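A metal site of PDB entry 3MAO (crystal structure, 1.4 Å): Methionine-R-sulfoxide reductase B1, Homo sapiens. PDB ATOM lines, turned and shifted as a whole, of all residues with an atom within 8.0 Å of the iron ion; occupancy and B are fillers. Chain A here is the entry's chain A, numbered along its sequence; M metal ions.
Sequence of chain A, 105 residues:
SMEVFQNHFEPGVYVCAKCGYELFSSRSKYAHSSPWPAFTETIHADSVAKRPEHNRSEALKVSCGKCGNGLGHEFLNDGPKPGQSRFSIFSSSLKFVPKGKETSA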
ATOM      1  N   VAL A  15      -1.355 -24.463 -16.393  1.00  0.00           N
ATOM      2  CA  VAL A  15      -0.531 -25.159 -15.481  1.00  0.00           C
ATOM      3  C   VAL A  15      -1.260 -25.437 -14.165  1.00  0.00           C
ATOM      4  O   VAL A  15      -2.277 -24.795 -13.843  1.00  0.00           O
ATOM      5  CB  VAL A  15       0.812 -24.445 -15.210  1.00  0.00           C
ATOM      6  CG1 VAL A  15       1.511 -24.148 -16.520  1.00  0.00           C
ATOM      7  CG2 VAL A  15       0.651 -23.157 -14.370  1.00  0.00           C
ATOM      8  N   CYS A  16      -0.741 -26.366 -13.347  1.00  0.00           N
ATOM      9  CA  CYS A  16      -1.285 -26.618 -12.016  1.00  0.00           C
ATOM     10  C   CYS A  16      -1.165 -25.344 -11.172  1.00  0.00           C
ATOM     11  O   CYS A  16      -0.090 -24.810 -11.026  1.00  0.00           O
ATOM     12  CB  CYS A  16      -0.516 -27.770 -11.376  1.00  0.00           C
ATOM     13  SG  CYS A  16      -1.041 -28.089  -9.679  1.00  0.00           S
ATOM     14  N   ALA A  17      -2.292 -24.889 -10.616  1.00  0.00           N
ATOM     15  CA  ALA A  17      -2.261 -23.683  -9.781  1.00  0.00           C
ATOM     16  C   ALA A  17      -1.407 -23.858  -8.539  1.00  0.00           C
ATOM     17  O   ALA A  17      -0.945 -22.837  -7.999  1.00  0.00           O
ATOM     18  CB  ALA A  17      -3.673 -23.255  -9.406  1.00  0.00           C
ATOM     19  N   LYS A  18      -1.213 -25.108  -8.081  1.00  0.00           N
ATOM     20  CA  LYS A  18      -0.477 -25.372  -6.868  1.00  0.00           C
ATOM     21  C   LYS A  18       1.008 -25.533  -7.084  1.00  0.00           C
ATOM     22  O   LYS A  18       1.788 -24.983  -6.298  1.00  0.00           O
ATOM     23  CB  LYS A  18      -1.031 -26.600  -6.153  1.00  0.00           C
ATOM     24  CG  LYS A  18      -0.402 -26.863  -4.794  1.00  0.00           C
ATOM     25  CD  LYS A  18      -1.186 -27.927  -4.022  1.00  0.00           C
ATOM     26  CE  LYS A  18      -0.460 -28.354  -2.754  1.00  0.00           C
ATOM     27  NZ  LYS A  18      -1.304 -29.306  -1.953  1.00  0.00           N
ATOM     28  N   CYS A  19       1.445 -26.214  -8.127  1.00  0.00           N
ATOM     29  CA  CYS A  19       2.886 -26.481  -8.279  1.00  0.00           C
ATOM     30  C   CYS A  19       3.486 -26.016  -9.607  1.00  0.00           C
ATOM     31  O   CYS A  19       4.691 -26.057  -9.795  1.00  0.00           O
ATOM     32  CB  CYS A  19       3.184 -27.983  -8.134  1.00  0.00           C
ATOM     33  SG  CYS A  19       2.693 -29.013  -9.540  1.00  0.00           S
ATOM     34  N   GLY A  20       2.652 -25.618 -10.563  1.00  0.00           N
ATOM     35  CA  GLY A  20       3.109 -25.115 -11.842  1.00  0.00           C
ATOM     36  C   GLY A  20       3.397 -26.154 -12.904  1.00  0.00           C
ATOM     37  O   GLY A  20       3.783 -25.781 -14.029  1.00  0.00           O
ATOM     38  N   TYR A  21       3.165 -27.427 -12.657  1.00  0.00           N
ATOM     39  CA  TYR A  21       3.386 -28.426 -13.701  1.00  0.00           C
ATOM     40  C   TYR A  21       2.440 -28.145 -14.869  1.00  0.00           C
ATOM     41  O   TYR A  21       1.301 -27.784 -14.686  1.00  0.00           O
ATOM     42  CB  TYR A  21       3.184 -29.869 -13.177  1.00  0.00           C
ATOM     43  CG  TYR A  21       3.827 -30.923 -14.018  1.00  0.00           C
ATOM     44  CD1 TYR A  21       3.153 -32.039 -14.401  1.00  0.00           C
ATOM     45  CD2 TYR A  21       5.181 -30.821 -14.356  1.00  0.00           C
ATOM     46  CE1 TYR A  21       3.785 -33.056 -15.141  1.00  0.00           C
ATOM     47  CE2 TYR A  21       5.802 -31.829 -15.095  1.00  0.00           C
ATOM     48  CZ  TYR A  21       5.102 -32.912 -15.470  1.00  0.00           C
ATOM     49  OH  TYR A  21       5.768 -33.901 -16.201  1.00  0.00           O
ATOM     50  N   GLU A  22       2.920 -28.354 -16.091  1.00  0.00           N
ATOM     51  CA  GLU A  22       2.094 -28.097 -17.273  1.00  0.00           C
ATOM     52  C   GLU A  22       1.052 -29.180 -17.436  1.00  0.00           C
ATOM     53  O   GLU A  22       1.363 -30.355 -17.413  1.00  0.00           O
ATOM     54  CB  GLU A  22       2.968 -27.978 -18.522  1.00  0.00           C
ATOM     55  CG  GLU A  22       4.103 -26.979 -18.438  1.00  0.00           C
ATOM     56  CD  GLU A  22       5.341 -27.466 -17.729  1.00  0.00           C
ATOM     57  OE1 GLU A  22       5.459 -28.678 -17.427  1.00  0.00           O
ATOM     58  OE2 GLU A  22       6.216 -26.598 -17.464  1.00  0.00           O
ATOM     59  N   LEU A  23      -0.204 -28.756 -17.583  1.00  0.00           N
ATOM     60  CA  LEU A  23      -1.360 -29.672 -17.660  1.00  0.00           C
ATOM     61  C   LEU A  23      -2.042 -29.726 -18.997  1.00  0.00           C
ATOM     62  O   LEU A  23      -2.185 -30.814 -19.535  1.00  0.00           O
ATOM     63  CB  LEU A  23      -2.388 -29.384 -16.546  1.00  0.00           C
ATOM     64  CG  LEU A  23      -1.852 -29.424 -15.119  1.00  0.00           C
ATOM     65  CD1 LEU A  23      -2.947 -28.992 -14.151  1.00  0.00           C
ATOM     66  CD2 LEU A  23      -1.322 -30.834 -14.760  1.00  0.00           C
ATOM     67  N   SER A  47       1.027 -35.642 -16.711  1.00  0.00           N
ATOM     68  CA  SER A  47       0.401 -34.427 -16.238  1.00  0.00           C
ATOM     69  C   SER A  47      -0.638 -34.704 -15.184  1.00  0.00           C
ATOM     70  O   SER A  47      -0.702 -33.962 -14.213  1.00  0.00           O
ATOM     71  CB  SER A  47      -0.258 -33.643 -17.374  1.00  0.00           C
ATOM     72  OG  SER A  47       0.711 -32.935 -18.157  1.00  0.00           O
ATOM     73  N   SER A  63      -6.193 -35.680 -10.917  1.00  0.00           N
ATOM     74  CA  SER A  63      -5.401 -34.823 -10.036  1.00  0.00           C
ATOM     75  C   SER A  63      -4.071 -34.512 -10.705  1.00  0.00           C
ATOM     76  O   SER A  63      -3.666 -35.212 -11.630  1.00  0.00           O
ATOM     77  CB  SER A  63      -5.172 -35.504  -8.676  1.00  0.00           C
ATOM     78  OG  SER A  63      -6.396 -35.875  -8.071  1.00  0.00           O
ATOM     79  N   CYS A  64      -3.358 -33.516 -10.203  1.00  0.00           N
ATOM     80  CA  CYS A  64      -2.057 -33.189 -10.738  1.00  0.00           C
ATOM     81  C   CYS A  64      -1.113 -34.362 -10.499  1.00  0.00           C
ATOM     82  O   CYS A  64      -1.015 -34.861  -9.407  1.00  0.00           O
ATOM     83  CB  CYS A  64      -1.514 -31.909 -10.115  1.00  0.00           C
ATOM     84  SG  CYS A  64       0.221 -31.543 -10.630  1.00  0.00           S
ATOM     85  N   GLY A  65      -0.407 -34.750 -11.548  1.00  0.00           N
ATOM     86  CA  GLY A  65       0.510 -35.893 -11.482  1.00  0.00           C
ATOM     87  C   GLY A  65       1.741 -35.638 -10.634  1.00  0.00           C
ATOM     88  O   GLY A  65       2.394 -36.613 -10.239  1.00  0.00           O
ATOM     89  N   LYS A  66       2.066 -34.365 -10.385  1.00  0.00           N
ATOM     90  CA  LYS A  66       3.233 -34.020  -9.579  1.00  0.00           C
ATOM     91  C   LYS A  66       2.915 -33.734  -8.135  1.00  0.00           C
ATOM     92  O   LYS A  66       3.620 -34.222  -7.244  1.00  0.00           O
ATOM     93  CB  LYS A  66       3.997 -32.877 -10.217  1.00  0.00           C
ATOM     94  CG  LYS A  66       4.623 -33.292 -11.503  1.00  0.00           C
ATOM     95  CD  LYS A  66       5.708 -34.379 -11.326  1.00  0.00           C
ATOM     96  CE  LYS A  66       6.627 -34.477 -12.533  1.00  0.00           C
ATOM     97  NZ  LYS A  66       7.651 -35.536 -12.363  1.00  0.00           N
ATOM     98  N   CYS A  67       1.864 -32.979  -7.851  1.00  0.00           N
ATOM     99  CA  CYS A  67       1.557 -32.624  -6.476  1.00  0.00           C
ATOM    100  C   CYS A  67       0.283 -33.198  -5.920  1.00  0.00           C
ATOM    101  O   CYS A  67       0.044 -33.035  -4.727  1.00  0.00           O
ATOM    102  CB  CYS A  67       1.526 -31.099  -6.284  1.00  0.00           C
ATOM    103  SG  CYS A  67       0.046 -30.288  -6.987  1.00  0.00           S
ATOM    104  N   GLY A  68      -0.556 -33.834  -6.738  1.00  0.00           N
ATOM    105  CA  GLY A  68      -1.785 -34.461  -6.249  1.00  0.00           C
ATOM    106  C   GLY A  68      -2.987 -33.541  -6.079  1.00  0.00           C
ATOM    107  O   GLY A  68      -4.048 -33.987  -5.649  1.00  0.00           O
ATOM    108  N   ASN A  69      -2.836 -32.260  -6.393  1.00  0.00           N
ATOM    109  CA  ASN A  69      -3.959 -31.368  -6.263  1.00  0.00           C
ATOM    110  C   ASN A  69      -5.121 -31.799  -7.170  1.00  0.00           C
ATOM    111  O   ASN A  69      -4.918 -32.130  -8.344  1.00  0.00           O
ATOM    112  CB  ASN A  69      -3.587 -29.924  -6.555  1.00  0.00           C
ATOM    113  CG  ASN A  69      -4.624 -28.952  -5.991  1.00  0.00           C
ATOM    114  OD1 ASN A  69      -5.053 -29.108  -4.850  1.00  0.00           O
ATOM    115  ND2 ASN A  69      -5.035 -28.040  -6.788  1.00  0.00           N
ATOM    116  N   GLY A  70      -6.326 -31.761  -6.640  1.00  0.00           N
ATOM    117  CA  GLY A  70      -7.486 -32.186  -7.383  1.00  0.00           C
ATOM    118  C   GLY A  70      -7.771 -31.246  -8.521  1.00  0.00           C
ATOM    119  O   GLY A  70      -7.707 -30.018  -8.379  1.00  0.00           O
ATOM    120  N   LEU A  71      -8.064 -31.817  -9.677  1.00  0.00           N
ATOM    121  CA  LEU A  71      -8.339 -31.044 -10.909  1.00  0.00           C
ATOM    122  C   LEU A  71      -9.755 -31.106 -11.406  1.00  0.00           C
ATOM    123  O   LEU A  71     -10.234 -30.132 -11.939  1.00  0.00           O
ATOM    124  CB  LEU A  71      -7.377 -31.492 -12.034  1.00  0.00           C
ATOM    125  CG  LEU A  71      -5.869 -31.389 -11.786  1.00  0.00           C
ATOM    126  CD1 LEU A  71      -5.155 -32.018 -12.988  1.00  0.00           C
ATOM    127  CD2 LEU A  71      -5.363 -30.002 -11.457  1.00  0.00           C
ATOM    128  N   SER A  93      -8.151 -24.799 -10.127  1.00  0.00           N
ATOM    129  CA  SER A  93      -7.024 -25.734 -10.115  1.00  0.00           C
ATOM    130  C   SER A  93      -5.964 -25.382 -11.174  1.00  0.00           C
ATOM    131  O   SER A  93      -4.928 -26.024 -11.234  1.00  0.00           O
ATOM    132  CB  SER A  93      -7.525 -27.153 -10.360  1.00  0.00           C
ATOM    133  OG  SER A  93      -8.372 -27.608  -9.290  1.00  0.00           O
HETATM  134 FE    FE M   1       0.544 -29.745  -9.165  1.00  0.00          FE
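The iron ion is bound by SG of Cys 67 (2.3 Å), SG of Cys 19 (2.3 Å), SG of Cys 64 (2.3 Å) and SG of Cys 16 (2.3 Å).
The nearest printed residue that does not touch the iron ion is Lys 18 (4.6 Å).
The side-chain sulfur (SG) of Cys 64 sits close to the backbone NH (N) of Lys 66 (3.4 Å). The backbone NH of Cys 64 sits at hydrogen-bond distance from the backbone carbonyl oxygen of Asn 69 (2.8 Å). The side-chain sulfur (SG) of Cys 19 lies close to the backbone NH (N) of Tyr 21, at 3.5 Å. The backbone NH of Lys 18 lies close to the side-chain sulfur of Cys 16, 3.4 Å away. The backbone NH of Asn 69 sits close to the side-chain sulfur of Cys 67. The backbone NH of Cys 16 lies within hydrogen-bond range of the backbone carbonyl oxygen of Tyr 21, at 2.8 Å.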
